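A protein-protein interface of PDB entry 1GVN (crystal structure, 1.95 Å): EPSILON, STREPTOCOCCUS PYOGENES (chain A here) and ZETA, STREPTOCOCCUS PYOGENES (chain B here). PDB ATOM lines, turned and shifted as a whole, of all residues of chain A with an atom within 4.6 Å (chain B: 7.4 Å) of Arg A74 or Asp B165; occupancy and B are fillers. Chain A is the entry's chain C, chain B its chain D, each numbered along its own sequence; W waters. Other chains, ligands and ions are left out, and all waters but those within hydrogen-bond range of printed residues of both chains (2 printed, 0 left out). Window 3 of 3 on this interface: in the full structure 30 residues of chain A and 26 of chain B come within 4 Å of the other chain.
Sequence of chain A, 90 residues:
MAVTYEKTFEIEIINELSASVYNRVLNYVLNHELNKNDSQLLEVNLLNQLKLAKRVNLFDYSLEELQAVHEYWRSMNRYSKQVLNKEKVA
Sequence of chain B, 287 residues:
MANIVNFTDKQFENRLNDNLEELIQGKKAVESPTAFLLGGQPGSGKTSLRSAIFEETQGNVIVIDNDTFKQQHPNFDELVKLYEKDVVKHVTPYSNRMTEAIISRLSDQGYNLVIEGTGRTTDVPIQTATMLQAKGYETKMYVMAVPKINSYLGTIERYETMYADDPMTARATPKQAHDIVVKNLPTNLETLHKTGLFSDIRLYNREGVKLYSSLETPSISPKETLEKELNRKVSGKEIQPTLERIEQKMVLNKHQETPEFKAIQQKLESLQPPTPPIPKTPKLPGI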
ATOM      1  N   ILE A  13      23.089 -16.779 -32.051  1.00  0.00           N
ATOM      2  CA  ILE A  13      22.781 -15.918 -30.914  1.00  0.00           C
ATOM      3  C   ILE A  13      23.900 -15.992 -29.876  1.00  0.00           C
ATOM      4  O   ILE A  13      24.327 -14.973 -29.334  1.00  0.00           O
ATOM      5  CB  ILE A  13      21.444 -16.327 -30.252  1.00  0.00           C
ATOM      6  CG1 ILE A  13      20.303 -16.211 -31.265  1.00  0.00           C
ATOM      7  CG2 ILE A  13      21.151 -15.416 -29.061  1.00  0.00           C
ATOM      8  CD1 ILE A  13      19.983 -14.775 -31.662  1.00  0.00           C
ATOM      9  N   LEU A  17      26.081 -12.822 -28.478  1.00  0.00           N
ATOM     10  CA  LEU A  17      26.043 -12.500 -27.055  1.00  0.00           C
ATOM     11  C   LEU A  17      27.399 -12.649 -26.372  1.00  0.00           C
ATOM     12  O   LEU A  17      27.814 -11.768 -25.617  1.00  0.00           O
ATOM     13  CB  LEU A  17      25.006 -13.367 -26.333  1.00  0.00           C
ATOM     14  CG  LEU A  17      24.839 -13.112 -24.829  1.00  0.00           C
ATOM     15  CD1 LEU A  17      24.481 -11.648 -24.582  1.00  0.00           C
ATOM     16  CD2 LEU A  17      23.744 -14.024 -24.280  1.00  0.00           C
ATOM     17  N   HIS A  70      23.888 -20.874 -23.883  1.00  0.00           N
ATOM     18  CA  HIS A  70      23.205 -19.608 -24.084  1.00  0.00           C
ATOM     19  C   HIS A  70      22.895 -18.980 -22.718  1.00  0.00           C
ATOM     20  O   HIS A  70      23.079 -17.775 -22.522  1.00  0.00           O
ATOM     21  CB  HIS A  70      21.925 -19.848 -24.886  1.00  0.00           C
ATOM     22  CG  HIS A  70      21.253 -18.598 -25.353  1.00  0.00           C
ATOM     23  ND1 HIS A  70      20.179 -18.614 -26.216  1.00  0.00           N
ATOM     24  CD2 HIS A  70      21.485 -17.296 -25.064  1.00  0.00           C
ATOM     25  CE1 HIS A  70      19.776 -17.375 -26.437  1.00  0.00           C
ATOM     26  NE2 HIS A  70      20.552 -16.557 -25.751  1.00  0.00           N
ATOM     27  N   GLU A  71      22.433 -19.791 -21.768  1.00  0.00           N
ATOM     28  CA  GLU A  71      22.133 -19.263 -20.434  1.00  0.00           C
ATOM     29  C   GLU A  71      23.428 -18.861 -19.733  1.00  0.00           C
ATOM     30  O   GLU A  71      23.460 -17.884 -18.986  1.00  0.00           O
ATOM     31  CB  GLU A  71      21.369 -20.294 -19.599  1.00  0.00           C
ATOM     32  CG  GLU A  71      21.086 -19.879 -18.151  1.00  0.00           C
ATOM     33  CD  GLU A  71      20.431 -18.511 -18.023  1.00  0.00           C
ATOM     34  OE1 GLU A  71      19.707 -18.094 -18.954  1.00  0.00           O
ATOM     35  OE2 GLU A  71      20.628 -17.850 -16.977  1.00  0.00           O
ATOM     36  N   TYR A  72      24.502 -19.604 -19.987  1.00  0.00           N
ATOM     37  CA  TYR A  72      25.793 -19.275 -19.384  1.00  0.00           C
ATOM     38  C   TYR A  72      26.157 -17.842 -19.748  1.00  0.00           C
ATOM     39  O   TYR A  72      26.564 -17.050 -18.895  1.00  0.00           O
ATOM     40  CB  TYR A  72      26.901 -20.209 -19.895  1.00  0.00           C
ATOM     41  CG  TYR A  72      28.299 -19.722 -19.539  1.00  0.00           C
ATOM     42  CD1 TYR A  72      28.879 -20.027 -18.307  1.00  0.00           C
ATOM     43  CD2 TYR A  72      29.016 -18.911 -20.421  1.00  0.00           C
ATOM     44  CE1 TYR A  72      30.147 -19.535 -17.962  1.00  0.00           C
ATOM     45  CE2 TYR A  72      30.271 -18.415 -20.087  1.00  0.00           C
ATOM     46  CZ  TYR A  72      30.831 -18.732 -18.861  1.00  0.00           C
ATOM     47  OH  TYR A  72      32.075 -18.248 -18.550  1.00  0.00           O
ATOM     48  N   TRP A  73      26.011 -17.504 -21.025  1.00  0.00           N
ATOM     49  CA  TRP A  73      26.355 -16.165 -21.463  1.00  0.00           C
ATOM     50  C   TRP A  73      25.360 -15.115 -20.988  1.00  0.00           C
ATOM     51  O   TRP A  73      25.729 -13.961 -20.810  1.00  0.00           O
ATOM     52  CB  TRP A  73      26.540 -16.130 -22.983  1.00  0.00           C
ATOM     53  CG  TRP A  73      27.797 -16.846 -23.403  1.00  0.00           C
ATOM     54  CD1 TRP A  73      27.888 -18.067 -24.008  1.00  0.00           C
ATOM     55  CD2 TRP A  73      29.143 -16.409 -23.180  1.00  0.00           C
ATOM     56  NE1 TRP A  73      29.207 -18.417 -24.174  1.00  0.00           N
ATOM     57  CE2 TRP A  73      29.997 -17.416 -23.675  1.00  0.00           C
ATOM     58  CE3 TRP A  73      29.709 -15.261 -22.608  1.00  0.00           C
ATOM     59  CZ2 TRP A  73      31.392 -17.313 -23.616  1.00  0.00           C
ATOM     60  CZ3 TRP A  73      31.097 -15.157 -22.549  1.00  0.00           C
ATOM     61  CH2 TRP A  73      31.922 -16.180 -23.051  1.00  0.00           C
ATOM     62  N   ARG A  74      24.106 -15.503 -20.774  1.00  0.00           N
ATOM     63  CA  ARG A  74      23.133 -14.541 -20.265  1.00  0.00           C
ATOM     64  C   ARG A  74      23.569 -14.215 -18.840  1.00  0.00           C
ATOM     65  O   ARG A  74      23.558 -13.055 -18.424  1.00  0.00           O
ATOM     66  CB  ARG A  74      21.717 -15.125 -20.207  1.00  0.00           C
ATOM     67  CG  ARG A  74      21.081 -15.460 -21.546  1.00  0.00           C
ATOM     68  CD  ARG A  74      19.556 -15.521 -21.400  1.00  0.00           C
ATOM     69  NE  ARG A  74      18.902 -16.120 -22.561  1.00  0.00           N
ATOM     70  CZ  ARG A  74      18.714 -17.427 -22.718  1.00  0.00           C
ATOM     71  NH1 ARG A  74      19.125 -18.278 -21.783  1.00  0.00           N
ATOM     72  NH2 ARG A  74      18.116 -17.889 -23.811  1.00  0.00           N
ATOM     73  N   SER A  75      23.958 -15.252 -18.097  1.00  0.00           N
ATOM     74  CA  SER A  75      24.387 -15.077 -16.713  1.00  0.00           C
ATOM     75  C   SER A  75      25.663 -14.248 -16.623  1.00  0.00           C
ATOM     76  O   SER A  75      25.797 -13.416 -15.731  1.00  0.00           O
ATOM     77  CB  SER A  75      24.597 -16.433 -16.020  1.00  0.00           C
ATOM     78  OG  SER A  75      25.753 -17.103 -16.500  1.00  0.00           O
ATOM     79  N   MET A  76      26.602 -14.471 -17.534  1.00  0.00           N
ATOM     80  CA  MET A  76      27.833 -13.693 -17.502  1.00  0.00           C
ATOM     81  C   MET A  76      27.576 -12.266 -17.986  1.00  0.00           C
ATOM     82  O   MET A  76      28.276 -11.338 -17.594  1.00  0.00           O
ATOM     83  CB  MET A  76      28.925 -14.364 -18.338  1.00  0.00           C
ATOM     84  CG  MET A  76      29.506 -15.609 -17.679  1.00  0.00           C
ATOM     85  SD  MET A  76      30.225 -15.267 -16.049  1.00  0.00           S
ATOM     86  CE  MET A  76      31.762 -16.228 -16.143  1.00  0.00           C
ATOM     87  N   ASN A  77      26.574 -12.088 -18.839  1.00  0.00           N
ATOM     88  CA  ASN A  77      26.248 -10.750 -19.313  1.00  0.00           C
ATOM     89  C   ASN A  77      25.815  -9.961 -18.074  1.00  0.00           C
ATOM     90  O   ASN A  77      26.298  -8.853 -17.826  1.00  0.00           O
ATOM     91  CB  ASN A  77      25.117 -10.806 -20.343  1.00  0.00           C
ATOM     92  CG  ASN A  77      24.810  -9.441 -20.954  1.00  0.00           C
ATOM     93  OD1 ASN A  77      25.714  -8.646 -21.225  1.00  0.00           O
ATOM     94  ND2 ASN A  77      23.526  -9.173 -21.187  1.00  0.00           N
ATOM     95  N   ARG A  78      24.927 -10.559 -17.284  1.00  0.00           N
ATOM     96  CA  ARG A  78      24.437  -9.925 -16.061  1.00  0.00           C
ATOM     97  C   ARG A  78      25.553  -9.716 -15.037  1.00  0.00           C
ATOM     98  O   ARG A  78      25.692  -8.632 -14.469  1.00  0.00           O
ATOM     99  CB  ARG A  78      23.338 -10.779 -15.417  1.00  0.00           C
ATOM    100  CG  ARG A  78      22.049 -10.899 -16.224  1.00  0.00           C
ATOM    101  CD  ARG A  78      20.950 -11.553 -15.384  1.00  0.00           C
ATOM    102  NE  ARG A  78      21.210 -12.958 -15.058  1.00  0.00           N
ATOM    103  CZ  ARG A  78      20.857 -13.984 -15.829  1.00  0.00           C
ATOM    104  NH1 ARG A  78      20.231 -13.771 -16.981  1.00  0.00           N
ATOM    105  NH2 ARG A  78      21.106 -15.227 -15.441  1.00  0.00           N
ATOM    106  N   TYR B 159      16.278 -10.587 -33.862  1.00  0.00           N
ATOM    107  CA  TYR B 159      16.093  -9.348 -33.104  1.00  0.00           C
ATOM    108  C   TYR B 159      15.333  -9.560 -31.794  1.00  0.00           C
ATOM    109  O   TYR B 159      15.785  -9.134 -30.731  1.00  0.00           O
ATOM    110  CB  TYR B 159      15.343  -8.311 -33.942  1.00  0.00           C
ATOM    111  CG  TYR B 159      14.865  -7.118 -33.129  1.00  0.00           C
ATOM    112  CD1 TYR B 159      15.776  -6.256 -32.514  1.00  0.00           C
ATOM    113  CD2 TYR B 159      13.505  -6.884 -32.936  1.00  0.00           C
ATOM    114  CE1 TYR B 159      15.343  -5.190 -31.722  1.00  0.00           C
ATOM    115  CE2 TYR B 159      13.058  -5.821 -32.146  1.00  0.00           C
ATOM    116  CZ  TYR B 159      13.982  -4.982 -31.542  1.00  0.00           C
ATOM    117  OH  TYR B 159      13.544  -3.950 -30.744  1.00  0.00           O
ATOM    118  N   GLU B 160      14.179 -10.216 -31.871  1.00  0.00           N
ATOM    119  CA  GLU B 160      13.361 -10.445 -30.682  1.00  0.00           C
ATOM    120  C   GLU B 160      14.100 -11.275 -29.643  1.00  0.00           C
ATOM    121  O   GLU B 160      13.947 -11.057 -28.440  1.00  0.00           O
ATOM    122  CB  GLU B 160      12.047 -11.138 -31.055  1.00  0.00           C
ATOM    123  CG  GLU B 160      11.154 -10.341 -32.004  1.00  0.00           C
ATOM    124  CD  GLU B 160      10.639  -9.043 -31.401  1.00  0.00           C
ATOM    125  OE1 GLU B 160      10.504  -8.965 -30.158  1.00  0.00           O
ATOM    126  OE2 GLU B 160      10.348  -8.104 -32.175  1.00  0.00           O
ATOM    127  N   THR B 161      14.908 -12.225 -30.104  1.00  0.00           N
ATOM    128  CA  THR B 161      15.660 -13.061 -29.183  1.00  0.00           C
ATOM    129  C   THR B 161      16.761 -12.249 -28.525  1.00  0.00           C
ATOM    130  O   THR B 161      16.976 -12.353 -27.320  1.00  0.00           O
ATOM    131  CB  THR B 161      16.280 -14.275 -29.894  1.00  0.00           C
ATOM    132  OG1 THR B 161      15.241 -15.060 -30.488  1.00  0.00           O
ATOM    133  CG2 THR B 161      17.051 -15.139 -28.897  1.00  0.00           C
ATOM    134  N   MET B 162      17.459 -11.433 -29.312  1.00  0.00           N
ATOM    135  CA  MET B 162      18.528 -10.604 -28.758  1.00  0.00           C
ATOM    136  C   MET B 162      17.915  -9.619 -27.771  1.00  0.00           C
ATOM    137  O   MET B 162      18.499  -9.314 -26.724  1.00  0.00           O
ATOM    138  CB  MET B 162      19.249  -9.834 -29.870  1.00  0.00           C
ATOM    139  CG  MET B 162      20.058 -10.707 -30.816  1.00  0.00           C
ATOM    140  SD  MET B 162      21.420 -11.543 -29.980  1.00  0.00           S
ATOM    141  CE  MET B 162      22.725 -10.321 -30.160  1.00  0.00           C
ATOM    142  N   TYR B 163      16.730  -9.123 -28.110  1.00  0.00           N
ATOM    143  CA  TYR B 163      16.033  -8.171 -27.257  1.00  0.00           C
ATOM    144  C   TYR B 163      15.738  -8.799 -25.901  1.00  0.00           C
ATOM    145  O   TYR B 163      15.915  -8.166 -24.862  1.00  0.00           O
ATOM    146  CB  TYR B 163      14.719  -7.742 -27.903  1.00  0.00           C
ATOM    147  CG  TYR B 163      14.008  -6.648 -27.143  1.00  0.00           C
ATOM    148  CD1 TYR B 163      14.375  -5.311 -27.300  1.00  0.00           C
ATOM    149  CD2 TYR B 163      12.979  -6.950 -26.252  1.00  0.00           C
ATOM    150  CE1 TYR B 163      13.729  -4.300 -26.589  1.00  0.00           C
ATOM    151  CE2 TYR B 163      12.329  -5.950 -25.537  1.00  0.00           C
ATOM    152  CZ  TYR B 163      12.707  -4.630 -25.708  1.00  0.00           C
ATOM    153  OH  TYR B 163      12.059  -3.642 -25.001  1.00  0.00           O
ATOM    154  N   ALA B 164      15.279 -10.045 -25.922  1.00  0.00           N
ATOM    155  CA  ALA B 164      14.960 -10.761 -24.695  1.00  0.00           C
ATOM    156  C   ALA B 164      16.216 -10.910 -23.841  1.00  0.00           C
ATOM    157  O   ALA B 164      16.151 -10.838 -22.613  1.00  0.00           O
ATOM    158  CB  ALA B 164      14.382 -12.132 -25.023  1.00  0.00           C
ATOM    159  N   ASP B 165      17.356 -11.103 -24.495  1.00  0.00           N
ATOM    160  CA  ASP B 165      18.623 -11.262 -23.790  1.00  0.00           C
ATOM    161  C   ASP B 165      19.150  -9.948 -23.228  1.00  0.00           C
ATOM    162  O   ASP B 165      19.593  -9.888 -22.079  1.00  0.00           O
ATOM    163  CB  ASP B 165      19.679 -11.871 -24.717  1.00  0.00           C
ATOM    164  CG  ASP B 165      19.455 -13.351 -24.968  1.00  0.00           C
ATOM    165  OD1 ASP B 165      18.510 -13.927 -24.388  1.00  0.00           O
ATOM    166  OD2 ASP B 165      20.233 -13.939 -25.744  1.00  0.00           O
ATOM    167  N   ASP B 166      19.110  -8.903 -24.045  1.00  0.00           N
ATOM    168  CA  ASP B 166      19.586  -7.594 -23.625  1.00  0.00           C
ATOM    169  C   ASP B 166      18.850  -6.499 -24.390  1.00  0.00           C
ATOM    170  O   ASP B 166      19.217  -6.165 -25.513  1.00  0.00           O
ATOM    171  CB  ASP B 166      21.088  -7.472 -23.881  1.00  0.00           C
ATOM    172  CG  ASP B 166      21.716  -6.347 -23.093  1.00  0.00           C
ATOM    173  OD1 ASP B 166      21.123  -5.246 -23.062  1.00  0.00           O
ATOM    174  OD2 ASP B 166      22.801  -6.561 -22.510  1.00  0.00           O
ATOM    175  N   PRO B 167      17.798  -5.929 -23.782  1.00  0.00           N
ATOM    176  CA  PRO B 167      16.964  -4.863 -24.354  1.00  0.00           C
ATOM    177  C   PRO B 167      17.774  -3.634 -24.753  1.00  0.00           C
ATOM    178  O   PRO B 167      17.362  -2.852 -25.610  1.00  0.00           O
ATOM    179  CB  PRO B 167      15.992  -4.535 -23.221  1.00  0.00           C
ATOM    180  CG  PRO B 167      15.911  -5.806 -22.452  1.00  0.00           C
ATOM    181  CD  PRO B 167      17.341  -6.272 -22.426  1.00  0.00           C
ATOM    182  N   MET B 168      18.928  -3.475 -24.117  1.00  0.00           N
ATOM    183  CA  MET B 168      19.810  -2.340 -24.353  1.00  0.00           C
ATOM    184  C   MET B 168      20.452  -2.303 -25.734  1.00  0.00           C
ATOM    185  O   MET B 168      20.324  -1.318 -26.460  1.00  0.00           O
ATOM    186  CB  MET B 168      20.926  -2.328 -23.304  1.00  0.00           C
ATOM    187  CG  MET B 168      21.164  -0.989 -22.631  1.00  0.00           C
ATOM    188  SD  MET B 168      19.903  -0.615 -21.394  1.00  0.00           S
ATOM    189  CE  MET B 168      20.434  -1.678 -20.042  1.00  0.00           C
ATOM    190  N   THR B 169      21.144  -3.379 -26.089  1.00  0.00           N
ATOM    191  CA  THR B 169      21.863  -3.447 -27.357  1.00  0.00           C
ATOM    192  C   THR B 169      21.150  -4.082 -28.548  1.00  0.00           C
ATOM    193  O   THR B 169      21.688  -4.086 -29.657  1.00  0.00           O
ATOM    194  CB  THR B 169      23.184  -4.193 -27.170  1.00  0.00           C
ATOM    195  OG1 THR B 169      22.910  -5.561 -26.838  1.00  0.00           O
ATOM    196  CG2 THR B 169      23.996  -3.557 -26.047  1.00  0.00           C
ATOM    197  N   ALA B 170      19.957  -4.624 -28.339  1.00  0.00           N
ATOM    198  CA  ALA B 170      19.239  -5.258 -29.439  1.00  0.00           C
ATOM    199  C   ALA B 170      18.818  -4.248 -30.500  1.00  0.00           C
ATOM    200  O   ALA B 170      18.280  -3.189 -30.182  1.00  0.00           O
ATOM    201  CB  ALA B 170      18.018  -5.999 -28.912  1.00  0.00           C
ATOM    202  N   ASN B 253       8.155  -9.846 -25.227  1.00  0.00           N
ATOM    203  CA  ASN B 253       8.905  -8.598 -25.349  1.00  0.00           C
ATOM    204  C   ASN B 253       7.999  -7.371 -25.394  1.00  0.00           C
ATOM    205  O   ASN B 253       8.481  -6.245 -25.536  1.00  0.00           O
ATOM    206  CB  ASN B 253       9.772  -8.603 -26.614  1.00  0.00           C
ATOM    207  CG  ASN B 253      10.941  -9.567 -26.525  1.00  0.00           C
ATOM    208  OD1 ASN B 253      11.375  -9.940 -25.432  1.00  0.00           O
ATOM    209  ND2 ASN B 253      11.471  -9.960 -27.680  1.00  0.00           N
HETATM  210  O   HOH W   1      16.640 -15.621 -25.137  1.00  0.00           O
HETATM  211  O   HOH W   2      21.579 -11.442 -20.792  1.00  0.00           O
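Of the 13 printed residues of chain B, 3 touch a printed residue of chain A. Printed residues of chain B that touch a printed residue of chain A: Met B162, Asp B165 and Asp B166. Along chain B the printed residues that touch a printed residue of chain A span positions 162 to 166.
A ring nitrogen (NE2) of His A70 lies within hydrogen-bond range of the side-chain carboxylate of Asp B165 (2.6 Å). The guanidinium group (NE) of Arg A74 is in salt-bridge range of the side-chain carboxylate (OD1) of Asp B165 (2.9 Å). OD2 of Asp B166 is in hydrogen-bond range of ND2 of Asn A77 (3.0 Å).
Of the printed residues of chain B, Ile A13 touches Met B162 and Asp B165. Of chain B, only Asp B165 (2.9 Å) comes within 4 Å of Arg A74. Printed residues of chain A within 4 Å of Met B162: Ile A13 (3.9 Å). Of chain A, only Ile A13 (3.7 Å), Leu A17 (3.8 Å), His A70 (2.6 Å) and Arg A74 (2.9 Å) come within 4 Å of Asp B165. Of the printed residues of chain A, Asp B166 touches Asn A77. The nearest residue of chain B that does not touch Arg A74 is Thr B161 (5.9 Å). The nearest residue of chain A that does not touch Asp B165 is Asn A77 (4.1 Å). The nearest printed residue of chain B that does not touch Asn A77 is Asp B165 (4.1 Å).
NH2 of Arg A74 sits close to ND1 of His A70 (3.3 Å). The side-chain carboxylate of Glu A71 is in salt-bridge range of the guanidinium group of Arg A74, 2.9 Å away. OD1 of Asp B166 lies close to N of Met B168, 3.0 Å away.
Among the printed residues, pairs that only touch across the chains: Ile A13 with Asp B165 (3.7 Å), Leu A17 with Asp B165 (3.8 Å) and Ile A13 with Met B162 (3.9 Å).
Water W1 bridges the side-chain carboxylate (OD1) of Asp B165 and the guanidinium group (NH2) of Arg A74. Water W2 lies within hydrogen-bond range of O of Asp B165 (2.8 Å), ND2 of Asn A77 (3.0 Å) and O of Arg A74 (3.5 Å).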
